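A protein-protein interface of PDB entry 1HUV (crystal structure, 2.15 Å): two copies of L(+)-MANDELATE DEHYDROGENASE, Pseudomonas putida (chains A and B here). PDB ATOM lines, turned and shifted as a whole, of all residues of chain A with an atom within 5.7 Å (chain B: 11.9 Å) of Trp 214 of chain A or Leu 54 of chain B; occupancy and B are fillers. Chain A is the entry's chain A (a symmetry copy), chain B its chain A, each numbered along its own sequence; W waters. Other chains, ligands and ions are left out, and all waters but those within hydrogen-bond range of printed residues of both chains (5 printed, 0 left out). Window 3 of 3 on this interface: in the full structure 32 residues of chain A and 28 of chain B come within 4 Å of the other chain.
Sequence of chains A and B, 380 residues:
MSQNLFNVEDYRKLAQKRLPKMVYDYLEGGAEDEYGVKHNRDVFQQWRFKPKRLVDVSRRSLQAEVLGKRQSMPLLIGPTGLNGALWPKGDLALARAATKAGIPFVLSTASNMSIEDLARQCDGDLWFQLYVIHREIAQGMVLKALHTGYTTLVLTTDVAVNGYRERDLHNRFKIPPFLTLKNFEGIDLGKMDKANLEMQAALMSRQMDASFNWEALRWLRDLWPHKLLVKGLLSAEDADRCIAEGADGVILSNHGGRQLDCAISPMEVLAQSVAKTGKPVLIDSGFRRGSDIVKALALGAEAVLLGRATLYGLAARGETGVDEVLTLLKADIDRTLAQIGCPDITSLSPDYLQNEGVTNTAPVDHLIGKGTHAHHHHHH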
ATOM      1  N   LEU A 155      30.663 -22.304 -13.173  1.00  0.00           N
ATOM      2  CA  LEU A 155      29.611 -21.601 -13.909  1.00  0.00           C
ATOM      3  C   LEU A 155      29.175 -20.401 -13.088  1.00  0.00           C
ATOM      4  O   LEU A 155      28.642 -20.570 -11.992  1.00  0.00           O
ATOM      5  CB  LEU A 155      28.395 -22.520 -14.101  1.00  0.00           C
ATOM      6  CG  LEU A 155      27.408 -22.393 -15.262  1.00  0.00           C
ATOM      7  CD1 LEU A 155      26.006 -22.605 -14.720  1.00  0.00           C
ATOM      8  CD2 LEU A 155      27.528 -21.058 -15.950  1.00  0.00           C
ATOM      9  N   THR A 157      26.596 -17.598 -12.541  1.00  0.00           N
ATOM     10  CA  THR A 157      25.216 -17.353 -12.906  1.00  0.00           C
ATOM     11  C   THR A 157      24.629 -16.009 -12.499  1.00  0.00           C
ATOM     12  O   THR A 157      23.425 -15.818 -12.661  1.00  0.00           O
ATOM     13  CB  THR A 157      24.344 -18.429 -12.256  1.00  0.00           C
ATOM     14  OG1 THR A 157      24.468 -18.324 -10.826  1.00  0.00           O
ATOM     15  CG2 THR A 157      24.803 -19.828 -12.681  1.00  0.00           C
ATOM     16  N   PHE A 212      19.744 -19.152 -19.582  1.00  0.00           N
ATOM     17  CA  PHE A 212      20.405 -20.295 -18.965  1.00  0.00           C
ATOM     18  C   PHE A 212      19.703 -20.620 -17.658  1.00  0.00           C
ATOM     19  O   PHE A 212      19.641 -19.790 -16.751  1.00  0.00           O
ATOM     20  CB  PHE A 212      21.886 -20.010 -18.726  1.00  0.00           C
ATOM     21  CG  PHE A 212      22.736 -21.250 -18.712  1.00  0.00           C
ATOM     22  CD1 PHE A 212      22.887 -22.005 -17.552  1.00  0.00           C
ATOM     23  CD2 PHE A 212      23.328 -21.702 -19.884  1.00  0.00           C
ATOM     24  CE1 PHE A 212      23.619 -23.192 -17.566  1.00  0.00           C
ATOM     25  CE2 PHE A 212      24.058 -22.884 -19.907  1.00  0.00           C
ATOM     26  CZ  PHE A 212      24.204 -23.633 -18.749  1.00  0.00           C
ATOM     27  N   ASN A 213      19.166 -21.835 -17.575  1.00  0.00           N
ATOM     28  CA  ASN A 213      18.430 -22.279 -16.397  1.00  0.00           C
ATOM     29  C   ASN A 213      18.846 -23.664 -15.919  1.00  0.00           C
ATOM     30  O   ASN A 213      19.855 -24.203 -16.361  1.00  0.00           O
ATOM     31  CB  ASN A 213      16.930 -22.269 -16.698  1.00  0.00           C
ATOM     32  CG  ASN A 213      16.569 -23.144 -17.883  1.00  0.00           C
ATOM     33  OD1 ASN A 213      17.406 -23.872 -18.413  1.00  0.00           O
ATOM     34  ND2 ASN A 213      15.305 -23.078 -18.299  1.00  0.00           N
ATOM     35  N   TRP A 214      18.054 -24.238 -15.017  1.00  0.00           N
ATOM     36  CA  TRP A 214      18.350 -25.552 -14.461  1.00  0.00           C
ATOM     37  C   TRP A 214      18.541 -26.626 -15.527  1.00  0.00           C
ATOM     38  O   TRP A 214      19.478 -27.420 -15.441  1.00  0.00           O
ATOM     39  CB  TRP A 214      17.258 -25.970 -13.472  1.00  0.00           C
ATOM     40  CG  TRP A 214      17.129 -25.017 -12.324  1.00  0.00           C
ATOM     41  CD1 TRP A 214      16.108 -24.148 -12.089  1.00  0.00           C
ATOM     42  CD2 TRP A 214      18.091 -24.804 -11.277  1.00  0.00           C
ATOM     43  NE1 TRP A 214      16.370 -23.399 -10.966  1.00  0.00           N
ATOM     44  CE2 TRP A 214      17.580 -23.777 -10.446  1.00  0.00           C
ATOM     45  CE3 TRP A 214      19.332 -25.378 -10.967  1.00  0.00           C
ATOM     46  CZ2 TRP A 214      18.269 -23.310  -9.324  1.00  0.00           C
ATOM     47  CZ3 TRP A 214      20.019 -24.911  -9.848  1.00  0.00           C
ATOM     48  CH2 TRP A 214      19.483 -23.883  -9.041  1.00  0.00           C
ATOM     49  N   GLU A 215      17.666 -26.652 -16.529  1.00  0.00           N
ATOM     50  CA  GLU A 215      17.792 -27.631 -17.601  1.00  0.00           C
ATOM     51  C   GLU A 215      19.144 -27.436 -18.285  1.00  0.00           C
ATOM     52  O   GLU A 215      19.847 -28.406 -18.579  1.00  0.00           O
ATOM     53  CB  GLU A 215      16.654 -27.463 -18.619  1.00  0.00           C
ATOM     54  CG  GLU A 215      16.710 -28.465 -19.767  1.00  0.00           C
ATOM     55  CD  GLU A 215      15.695 -28.196 -20.848  1.00  0.00           C
ATOM     56  OE1 GLU A 215      15.206 -27.050 -20.946  1.00  0.00           O
ATOM     57  OE2 GLU A 215      15.388 -29.128 -21.629  1.00  0.00           O
ATOM     58  N   ALA A 216      19.506 -26.180 -18.531  1.00  0.00           N
ATOM     59  CA  ALA A 216      20.777 -25.856 -19.172  1.00  0.00           C
ATOM     60  C   ALA A 216      21.962 -26.316 -18.323  1.00  0.00           C
ATOM     61  O   ALA A 216      23.013 -26.687 -18.860  1.00  0.00           O
ATOM     62  CB  ALA A 216      20.859 -24.352 -19.432  1.00  0.00           C
ATOM     63  N   LEU A 217      21.785 -26.301 -17.001  1.00  0.00           N
ATOM     64  CA  LEU A 217      22.836 -26.725 -16.072  1.00  0.00           C
ATOM     65  C   LEU A 217      23.080 -28.227 -16.241  1.00  0.00           C
ATOM     66  O   LEU A 217      24.214 -28.685 -16.133  1.00  0.00           O
ATOM     67  CB  LEU A 217      22.422 -26.440 -14.617  1.00  0.00           C
ATOM     68  CG  LEU A 217      23.443 -26.174 -13.505  1.00  0.00           C
ATOM     69  CD1 LEU A 217      22.904 -26.759 -12.217  1.00  0.00           C
ATOM     70  CD2 LEU A 217      24.786 -26.775 -13.822  1.00  0.00           C
ATOM     71  N   ARG A 218      22.011 -28.985 -16.480  1.00  0.00           N
ATOM     72  CA  ARG A 218      22.122 -30.431 -16.673  1.00  0.00           C
ATOM     73  C   ARG A 218      22.965 -30.657 -17.919  1.00  0.00           C
ATOM     74  O   ARG A 218      23.843 -31.516 -17.948  1.00  0.00           O
ATOM     75  CB  ARG A 218      20.750 -31.064 -16.897  1.00  0.00           C
ATOM     76  CG  ARG A 218      19.775 -30.983 -15.741  1.00  0.00           C
ATOM     77  CD  ARG A 218      18.457 -31.634 -16.156  1.00  0.00           C
ATOM     78  NE  ARG A 218      17.401 -31.502 -15.165  1.00  0.00           N
ATOM     79  CZ  ARG A 218      16.934 -30.343 -14.710  1.00  0.00           C
ATOM     80  NH1 ARG A 218      17.438 -29.201 -15.156  1.00  0.00           N
ATOM     81  NH2 ARG A 218      15.947 -30.330 -13.822  1.00  0.00           N
ATOM     82  N   TRP A 219      22.668 -29.883 -18.957  1.00  0.00           N
ATOM     83  CA  TRP A 219      23.396 -29.966 -20.213  1.00  0.00           C
ATOM     84  C   TRP A 219      24.880 -29.779 -19.931  1.00  0.00           C
ATOM     85  O   TRP A 219      25.710 -30.581 -20.364  1.00  0.00           O
ATOM     86  CB  TRP A 219      22.904 -28.876 -21.170  1.00  0.00           C
ATOM     87  CG  TRP A 219      23.796 -28.659 -22.348  1.00  0.00           C
ATOM     88  CD1 TRP A 219      23.921 -29.456 -23.444  1.00  0.00           C
ATOM     89  CD2 TRP A 219      24.723 -27.574 -22.527  1.00  0.00           C
ATOM     90  NE1 TRP A 219      24.869 -28.941 -24.301  1.00  0.00           N
ATOM     91  CE2 TRP A 219      25.379 -27.788 -23.766  1.00  0.00           C
ATOM     92  CE3 TRP A 219      25.061 -26.448 -21.761  1.00  0.00           C
ATOM     93  CZ2 TRP A 219      26.354 -26.916 -24.256  1.00  0.00           C
ATOM     94  CZ3 TRP A 219      26.032 -25.579 -22.248  1.00  0.00           C
ATOM     95  CH2 TRP A 219      26.668 -25.820 -23.486  1.00  0.00           C
ATOM     96  N   VAL A 230      28.907 -24.140  -9.108  1.00  0.00           N
ATOM     97  CA  VAL A 230      28.006 -23.090  -9.574  1.00  0.00           C
ATOM     98  C   VAL A 230      28.264 -21.878  -8.689  1.00  0.00           C
ATOM     99  O   VAL A 230      28.119 -21.948  -7.464  1.00  0.00           O
ATOM    100  CB  VAL A 230      26.535 -23.501  -9.455  1.00  0.00           C
ATOM    101  CG1 VAL A 230      25.633 -22.328  -9.863  1.00  0.00           C
ATOM    102  CG2 VAL A 230      26.269 -24.715 -10.314  1.00  0.00           C
ATOM    103  N   LEU A 233      25.491 -17.895  -6.172  1.00  0.00           N
ATOM    104  CA  LEU A 233      24.334 -18.270  -5.370  1.00  0.00           C
ATOM    105  C   LEU A 233      24.186 -17.452  -4.090  1.00  0.00           C
ATOM    106  O   LEU A 233      25.178 -17.075  -3.466  1.00  0.00           O
ATOM    107  CB  LEU A 233      24.411 -19.761  -5.021  1.00  0.00           C
ATOM    108  CG  LEU A 233      24.516 -20.729  -6.195  1.00  0.00           C
ATOM    109  CD1 LEU A 233      24.368 -22.153  -5.685  1.00  0.00           C
ATOM    110  CD2 LEU A 233      23.432 -20.410  -7.220  1.00  0.00           C
ATOM    111  N   ASP A 238      18.921 -22.548  -3.380  1.00  0.00           N
ATOM    112  CA  ASP A 238      19.547 -22.601  -4.696  1.00  0.00           C
ATOM    113  C   ASP A 238      20.786 -23.500  -4.641  1.00  0.00           C
ATOM    114  O   ASP A 238      21.037 -24.277  -5.560  1.00  0.00           O
ATOM    115  CB  ASP A 238      19.962 -21.200  -5.165  1.00  0.00           C
ATOM    116  CG  ASP A 238      18.875 -20.497  -5.947  1.00  0.00           C
ATOM    117  OD1 ASP A 238      17.810 -21.104  -6.188  1.00  0.00           O
ATOM    118  OD2 ASP A 238      19.083 -19.326  -6.337  1.00  0.00           O
ATOM    119  N   ARG A 241      19.678 -27.071  -4.703  1.00  0.00           N
ATOM    120  CA  ARG A 241      19.160 -27.467  -6.009  1.00  0.00           C
ATOM    121  C   ARG A 241      20.348 -27.752  -6.930  1.00  0.00           C
ATOM    122  O   ARG A 241      20.342 -28.721  -7.690  1.00  0.00           O
ATOM    123  CB  ARG A 241      18.273 -26.345  -6.571  1.00  0.00           C
ATOM    124  CG  ARG A 241      17.749 -26.538  -8.001  1.00  0.00           C
ATOM    125  CD  ARG A 241      16.739 -27.666  -8.110  1.00  0.00           C
ATOM    126  NE  ARG A 241      16.298 -27.907  -9.482  1.00  0.00           N
ATOM    127  CZ  ARG A 241      15.336 -27.232 -10.106  1.00  0.00           C
ATOM    128  NH1 ARG A 241      14.689 -26.250  -9.489  1.00  0.00           N
ATOM    129  NH2 ARG A 241      15.013 -27.558 -11.351  1.00  0.00           N
ATOM    130  N   CYS A 242      21.374 -26.906  -6.851  1.00  0.00           N
ATOM    131  CA  CYS A 242      22.568 -27.096  -7.663  1.00  0.00           C
ATOM    132  C   CYS A 242      23.160 -28.483  -7.400  1.00  0.00           C
ATOM    133  O   CYS A 242      23.524 -29.195  -8.339  1.00  0.00           O
ATOM    134  CB  CYS A 242      23.601 -26.015  -7.350  1.00  0.00           C
ATOM    135  SG  CYS A 242      23.279 -24.435  -8.151  1.00  0.00           S
ATOM    136  N   GLU A 245      21.097 -31.178  -8.915  1.00  0.00           N
ATOM    137  CA  GLU A 245      21.249 -31.222 -10.362  1.00  0.00           C
ATOM    138  C   GLU A 245      22.625 -31.723 -10.803  1.00  0.00           C
ATOM    139  O   GLU A 245      22.931 -31.735 -11.998  1.00  0.00           O
ATOM    140  CB  GLU A 245      20.986 -29.837 -10.958  1.00  0.00           C
ATOM    141  CG  GLU A 245      19.572 -29.288 -10.706  1.00  0.00           C
ATOM    142  CD  GLU A 245      18.501 -29.987 -11.509  1.00  0.00           C
ATOM    143  OE1 GLU A 245      18.827 -30.892 -12.306  1.00  0.00           O
ATOM    144  OE2 GLU A 245      17.311 -29.632 -11.354  1.00  0.00           O
ATOM    145  N   LYS B  50      17.415 -11.835  -2.059  1.00  0.00           N
ATOM    146  CA  LYS B  50      17.885 -13.206  -2.095  1.00  0.00           C
ATOM    147  C   LYS B  50      17.431 -13.643  -3.480  1.00  0.00           C
ATOM    148  O   LYS B  50      16.342 -14.194  -3.648  1.00  0.00           O
ATOM    149  CB  LYS B  50      17.203 -14.058  -1.019  1.00  0.00           C
ATOM    150  CG  LYS B  50      17.458 -13.563   0.397  1.00  0.00           C
ATOM    151  CD  LYS B  50      18.030 -14.652   1.296  1.00  0.00           C
ATOM    152  CE  LYS B  50      17.071 -15.818   1.461  1.00  0.00           C
ATOM    153  NZ  LYS B  50      17.606 -16.835   2.411  1.00  0.00           N
ATOM    154  N   PRO B  51      18.241 -13.347  -4.502  1.00  0.00           N
ATOM    155  CA  PRO B  51      17.834 -13.752  -5.847  1.00  0.00           C
ATOM    156  C   PRO B  51      17.763 -15.250  -6.067  1.00  0.00           C
ATOM    157  O   PRO B  51      18.397 -16.036  -5.354  1.00  0.00           O
ATOM    158  CB  PRO B  51      18.863 -13.069  -6.758  1.00  0.00           C
ATOM    159  CG  PRO B  51      19.994 -12.693  -5.854  1.00  0.00           C
ATOM    160  CD  PRO B  51      19.346 -12.373  -4.544  1.00  0.00           C
ATOM    161  N   LYS B  52      16.959 -15.631  -7.053  1.00  0.00           N
ATOM    162  CA  LYS B  52      16.785 -17.024  -7.430  1.00  0.00           C
ATOM    163  C   LYS B  52      17.589 -17.188  -8.716  1.00  0.00           C
ATOM    164  O   LYS B  52      17.262 -16.590  -9.740  1.00  0.00           O
ATOM    165  CB  LYS B  52      15.299 -17.320  -7.672  1.00  0.00           C
ATOM    166  CG  LYS B  52      14.408 -17.039  -6.459  1.00  0.00           C
ATOM    167  CD  LYS B  52      12.968 -17.489  -6.691  1.00  0.00           C
ATOM    168  CE  LYS B  52      12.083 -17.189  -5.482  1.00  0.00           C
ATOM    169  NZ  LYS B  52      12.636 -17.742  -4.213  1.00  0.00           N
ATOM    170  N   ARG B  53      18.655 -17.977  -8.653  1.00  0.00           N
ATOM    171  CA  ARG B  53      19.515 -18.184  -9.813  1.00  0.00           C
ATOM    172  C   ARG B  53      19.026 -19.275 -10.761  1.00  0.00           C
ATOM    173  O   ARG B  53      18.173 -20.090 -10.412  1.00  0.00           O
ATOM    174  CB  ARG B  53      20.940 -18.522  -9.367  1.00  0.00           C
ATOM    175  CG  ARG B  53      21.657 -17.410  -8.614  1.00  0.00           C
ATOM    176  CD  ARG B  53      21.817 -16.160  -9.461  1.00  0.00           C
ATOM    177  NE  ARG B  53      22.458 -15.095  -8.700  1.00  0.00           N
ATOM    178  CZ  ARG B  53      22.090 -13.822  -8.748  1.00  0.00           C
ATOM    179  NH1 ARG B  53      21.083 -13.454  -9.526  1.00  0.00           N
ATOM    180  NH2 ARG B  53      22.715 -12.920  -8.005  1.00  0.00           N
ATOM    181  N   LEU B  54      19.589 -19.268 -11.965  1.00  0.00           N
ATOM    182  CA  LEU B  54      19.264 -20.236 -12.999  1.00  0.00           C
ATOM    183  C   LEU B  54      17.801 -20.228 -13.412  1.00  0.00           C
ATOM    184  O   LEU B  54      17.208 -21.265 -13.719  1.00  0.00           O
ATOM    185  CB  LEU B  54      19.716 -21.629 -12.560  1.00  0.00           C
ATOM    186  CG  LEU B  54      21.251 -21.659 -12.560  1.00  0.00           C
ATOM    187  CD1 LEU B  54      21.777 -22.823 -11.744  1.00  0.00           C
ATOM    188  CD2 LEU B  54      21.746 -21.720 -14.000  1.00  0.00           C
ATOM    189  N   VAL B  55      17.227 -19.031 -13.411  1.00  0.00           N
ATOM    190  CA  VAL B  55      15.855 -18.845 -13.839  1.00  0.00           C
ATOM    191  C   VAL B  55      15.980 -18.138 -15.172  1.00  0.00           C
ATOM    192  O   VAL B  55      16.812 -17.240 -15.336  1.00  0.00           O
ATOM    193  CB  VAL B  55      15.057 -17.953 -12.877  1.00  0.00           C
ATOM    194  CG1 VAL B  55      13.657 -17.709 -13.437  1.00  0.00           C
ATOM    195  CG2 VAL B  55      14.968 -18.612 -11.512  1.00  0.00           C
ATOM    196  N   ASP B  56      15.171 -18.568 -16.130  1.00  0.00           N
ATOM    197  CA  ASP B  56      15.168 -17.984 -17.457  1.00  0.00           C
ATOM    198  C   ASP B  56      14.532 -16.606 -17.377  1.00  0.00           C
ATOM    199  O   ASP B  56      13.325 -16.485 -17.178  1.00  0.00           O
ATOM    200  CB  ASP B  56      14.369 -18.885 -18.404  1.00  0.00           C
ATOM    201  CG  ASP B  56      14.197 -18.288 -19.789  1.00  0.00           C
ATOM    202  OD1 ASP B  56      14.714 -17.182 -20.049  1.00  0.00           O
ATOM    203  OD2 ASP B  56      13.531 -18.937 -20.622  1.00  0.00           O
ATOM    204  N   VAL B  57      15.345 -15.566 -17.512  1.00  0.00           N
ATOM    205  CA  VAL B  57      14.823 -14.210 -17.464  1.00  0.00           C
ATOM    206  C   VAL B  57      15.090 -13.481 -18.776  1.00  0.00           C
ATOM    207  O   VAL B  57      15.251 -12.261 -18.802  1.00  0.00           O
ATOM    208  CB  VAL B  57      15.424 -13.417 -16.272  1.00  0.00           C
ATOM    209  CG1 VAL B  57      15.011 -14.078 -14.966  1.00  0.00           C
ATOM    210  CG2 VAL B  57      16.946 -13.344 -16.383  1.00  0.00           C
ATOM    211  N   SER B  58      15.120 -14.241 -19.869  1.00  0.00           N
ATOM    212  CA  SER B  58      15.359 -13.672 -21.197  1.00  0.00           C
ATOM    213  C   SER B  58      14.151 -12.884 -21.692  1.00  0.00           C
ATOM    214  O   SER B  58      14.274 -12.039 -22.575  1.00  0.00           O
ATOM    215  CB  SER B  58      15.688 -14.782 -22.199  1.00  0.00           C
ATOM    216  OG  SER B  58      14.598 -15.682 -22.334  1.00  0.00           O
ATOM    217  N   ARG B  59      12.984 -13.176 -21.130  1.00  0.00           N
ATOM    218  CA  ARG B  59      11.752 -12.483 -21.501  1.00  0.00           C
ATOM    219  C   ARG B  59      11.106 -11.993 -20.205  1.00  0.00           C
ATOM    220  O   ARG B  59      10.584 -12.791 -19.427  1.00  0.00           O
ATOM    221  CB  ARG B  59      10.796 -13.439 -22.228  1.00  0.00           C
ATOM    222  CG  ARG B  59      11.388 -14.145 -23.451  1.00  0.00           C
ATOM    223  CD  ARG B  59      10.318 -14.987 -24.148  1.00  0.00           C
ATOM    224  NE  ARG B  59      10.773 -15.591 -25.401  1.00  0.00           N
ATOM    225  CZ  ARG B  59      11.710 -16.531 -25.491  1.00  0.00           C
ATOM    226  NH1 ARG B  59      12.308 -16.988 -24.397  1.00  0.00           N
ATOM    227  NH2 ARG B  59      12.044 -17.026 -26.677  1.00  0.00           N
ATOM    228  N   LEU B 337      14.455  -7.065 -11.714  1.00  0.00           N
ATOM    229  CA  LEU B 337      13.708  -8.300 -11.855  1.00  0.00           C
ATOM    230  C   LEU B 337      14.631  -9.380 -12.425  1.00  0.00           C
ATOM    231  O   LEU B 337      14.654 -10.501 -11.931  1.00  0.00           O
ATOM    232  CB  LEU B 337      12.487  -8.084 -12.762  1.00  0.00           C
ATOM    233  CG  LEU B 337      11.383  -7.174 -12.208  1.00  0.00           C
ATOM    234  CD1 LEU B 337      10.241  -7.094 -13.210  1.00  0.00           C
ATOM    235  CD2 LEU B 337      10.876  -7.711 -10.870  1.00  0.00           C
ATOM    236  N   ALA B 338      15.409  -9.037 -13.448  1.00  0.00           N
ATOM    237  CA  ALA B 338      16.323 -10.004 -14.052  1.00  0.00           C
ATOM    238  C   ALA B 338      17.318 -10.519 -13.020  1.00  0.00           C
ATOM    239  O   ALA B 338      17.533 -11.725 -12.889  1.00  0.00           O
ATOM    240  CB  ALA B 338      17.080  -9.367 -15.212  1.00  0.00           C
ATOM    241  N   GLN B 339      17.911  -9.587 -12.287  1.00  0.00           N
ATOM    242  CA  GLN B 339      18.906  -9.906 -11.278  1.00  0.00           C
ATOM    243  C   GLN B 339      18.424 -10.769 -10.121  1.00  0.00           C
ATOM    244  O   GLN B 339      19.201 -11.552  -9.578  1.00  0.00           O
ATOM    245  CB  GLN B 339      19.526  -8.613 -10.757  1.00  0.00           C
ATOM    246  CG  GLN B 339      20.514  -8.002 -11.737  1.00  0.00           C
ATOM    247  CD  GLN B 339      20.692  -6.516 -11.534  1.00  0.00           C
ATOM    248  OE1 GLN B 339      21.683  -5.932 -11.970  1.00  0.00           O
ATOM    249  NE2 GLN B 339      19.720  -5.889 -10.885  1.00  0.00           N
ATOM    250  N   ILE B 340      17.157 -10.638  -9.731  1.00  0.00           N
ATOM    251  CA  ILE B 340      16.647 -11.457  -8.635  1.00  0.00           C
ATOM    252  C   ILE B 340      15.927 -12.700  -9.160  1.00  0.00           C
ATOM    253  O   ILE B 340      15.434 -13.524  -8.387  1.00  0.00           O
ATOM    254  CB  ILE B 340      15.694 -10.654  -7.689  1.00  0.00           C
ATOM    255  CG1 ILE B 340      14.395 -10.284  -8.413  1.00  0.00           C
ATOM    256  CG2 ILE B 340      16.411  -9.408  -7.174  1.00  0.00           C
ATOM    257  CD1 ILE B 340      13.325  -9.693  -7.490  1.00  0.00           C
ATOM    258  N   GLY B 341      15.874 -12.836 -10.480  1.00  0.00           N
ATOM    259  CA  GLY B 341      15.236 -13.999 -11.072  1.00  0.00           C
ATOM    260  C   GLY B 341      13.721 -14.064 -11.014  1.00  0.00           C
ATOM    261  O   GLY B 341      13.154 -15.140 -10.826  1.00  0.00           O
ATOM    262  N   CYS B 342      13.060 -12.920 -11.158  1.00  0.00           N
ATOM    263  CA  CYS B 342      11.600 -12.885 -11.163  1.00  0.00           C
ATOM    264  C   CYS B 342      11.253 -12.176 -12.465  1.00  0.00           C
ATOM    265  O   CYS B 342      10.982 -10.975 -12.480  1.00  0.00           O
ATOM    266  CB  CYS B 342      11.065 -12.101  -9.962  1.00  0.00           C
ATOM    267  SG  CYS B 342       9.273 -12.228  -9.719  1.00  0.00           S
ATOM    268  N   PRO B 343      11.271 -12.916 -13.586  1.00  0.00           N
ATOM    269  CA  PRO B 343      10.966 -12.339 -14.898  1.00  0.00           C
ATOM    270  C   PRO B 343       9.638 -11.599 -14.996  1.00  0.00           C
ATOM    271  O   PRO B 343       9.554 -10.561 -15.651  1.00  0.00           O
ATOM    272  CB  PRO B 343      11.043 -13.546 -15.836  1.00  0.00           C
ATOM    273  CG  PRO B 343      10.663 -14.691 -14.953  1.00  0.00           C
ATOM    274  CD  PRO B 343      11.417 -14.380 -13.681  1.00  0.00           C
ATOM    275  N   TYR B 352      11.637 -13.252  -2.155  1.00  0.00           N
ATOM    276  CA  TYR B 352      12.838 -12.669  -2.726  1.00  0.00           C
ATOM    277  C   TYR B 352      13.553 -11.739  -1.756  1.00  0.00           C
ATOM    278  O   TYR B 352      14.600 -11.189  -2.084  1.00  0.00           O
ATOM    279  CB  TYR B 352      12.494 -11.903  -4.006  1.00  0.00           C
ATOM    280  CG  TYR B 352      11.957 -12.777  -5.115  1.00  0.00           C
ATOM    281  CD1 TYR B 352      10.612 -13.155  -5.150  1.00  0.00           C
ATOM    282  CD2 TYR B 352      12.802 -13.257  -6.113  1.00  0.00           C
ATOM    283  CE1 TYR B 352      10.126 -13.992  -6.155  1.00  0.00           C
ATOM    284  CE2 TYR B 352      12.328 -14.093  -7.119  1.00  0.00           C
ATOM    285  CZ  TYR B 352      10.994 -14.456  -7.135  1.00  0.00           C
ATOM    286  OH  TYR B 352      10.531 -15.286  -8.127  1.00  0.00           O
HETATM  287  O   HOH W   1      16.390 -20.426  -8.590  1.00  0.00           O
HETATM  288  O   HOH W   2      19.403 -17.175 -15.664  1.00  0.00           O
HETATM  289  O   HOH W   3      21.083 -17.227 -13.352  1.00  0.00           O
HETATM  290  O   HOH W   4      17.239 -18.210  -3.971  1.00  0.00           O
HETATM  291  O   HOH W   5      20.710 -17.631  -5.228  1.00  0.00           O
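O of Gln 339 of chain B lies within hydrogen-bond range of NH1 of Arg 53 of chain B (2.7 Å). O of Trp 214 of chain A sits at hydrogen-bond distance from NH1 of Arg 218 of chain A (2.7 Å). N of Glu 215 of chain A sits close to OD1 of Asn 213 of chain A, at 3.4 Å. The backbone NH of Ala 216 of chain A is in hydrogen-bond range of the side-chain amide oxygen of Asn 213 of chain A, at 3.1 Å. N of Lys 52 of chain B sits at hydrogen-bond distance from O of Ile 340 of chain B (2.9 Å).
Leu 54 of chain B touches just these residues of chain A: Thr 157 (3.8 Å), Phe 212 (3.7 Å), Asn 213 (3.1 Å) and Trp 214 (3.3 Å). Phe 212 of chain A touches just one residue of chain B: Leu 54 (3.7 Å). Asn 213 of chain A touches one residue of chain B. No residue of chain B comes within 4 Å of Glu 215 of chain A. No residue of chain B comes within 4 Å of Ala 216 of chain A. Arg 218 of chain A touches none of the printed residues of chain B. No residue of chain B comes within 4 Å of Val 230 of chain A. No residue of chain B comes within 4 Å of Arg 241 of chain A. No residue of chain B comes within 4 Å of Glu 245 of chain A. Of the printed residues of chain A, Pro 51 of chain B touches Asp 238 (3.5 Å). Of the printed residues of chain A, Lys 52 of chain B touches Asp 238 (3.4 Å). Of the printed residues of chain A, Arg 53 of chain B touches Thr 157, Trp 214, Leu 233 and Asp 238. Printed residues of chain B within 4 Å of Leu 233 of chain A: Arg 53 (3.8 Å). The nearest residue of chain A that does not touch Leu 54 of chain B is Leu 217 of chain A (4.1 Å). The nearest printed residue of chain B that does not touch Leu 233 of chain A is Leu 54 of chain B (5.4 Å).
No position is printed for both chains. Of the 10 pairs that touch across the chains among the printed residues, none has its exchanged pair printed and touching as well.
Printed residues of chain B that touch a printed residue of chain A: Pro 51, Lys 52, Arg 53 and Leu 54. Hydrophobic or aromatic side chains of chain B that line the printed part of chain A: Leu 54. Of the 16 printed residues of chain A, 6 touch a printed residue of chain B. Printed residues of chain A that touch a printed residue of chain B: Thr 157, Phe 212, Asn 213, Trp 214, Leu 233 and Asp 238. Hydrophobic or aromatic side chains of chain A within 4 Å of the printed part of chain B: Phe 212, Trp 214 and Leu 233.
Water W1 bridges O of Arg 53 of chain B (2.6 Å) and OD1 of Asp 238 of chain A (2.9 Å). Water W5 lies within hydrogen-bond range of OD2 of Asp 238 of chain A and O of Pro 51 of chain B. Water W2 bridges the backbone carbonyl oxygen of Val 55 of chain B (2.6 Å) and the backbone carbonyl oxygen of Phe 212 of chain A (2.8 Å). Water W3 bridges O of Thr 157 of chain A and N of Leu 54 of chain B. Water W4 lies within hydrogen-bond range of O of Pro 51 of chain B (2.8 Å) and OD2 of Asp 238 of chain A (3.2 Å).
Among the printed residues, pairs that only touch across the chains: Asn 213 of chain A with Leu 54 of chain B (3.1 Å), Trp 214 of chain A with Arg 53 of chain B (3.4 Å), Asp 238 of chain A with Lys 52 of chain B (3.4 Å), Asp 238 of chain A with Pro 51 of chain B (3.5 Å), Thr 157 of chain A with Arg 53 of chain B (3.6 Å), Phe 212 of chain A with Leu 54 of chain B (3.7 Å), Leu 233 of chain A with Arg 53 of chain B (3.8 Å) and Thr 157 of chain A with Leu 54 of chain B (3.8 Å).
O of Leu 54 of chain B lies within hydrogen-bond range of N of Trp 214 of chain A. The backbone NH (N) of Arg 53 of chain B lies within hydrogen-bond range of the side-chain carboxylate (OD2) of Asp 238 of chain A, at 2.7 Å.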
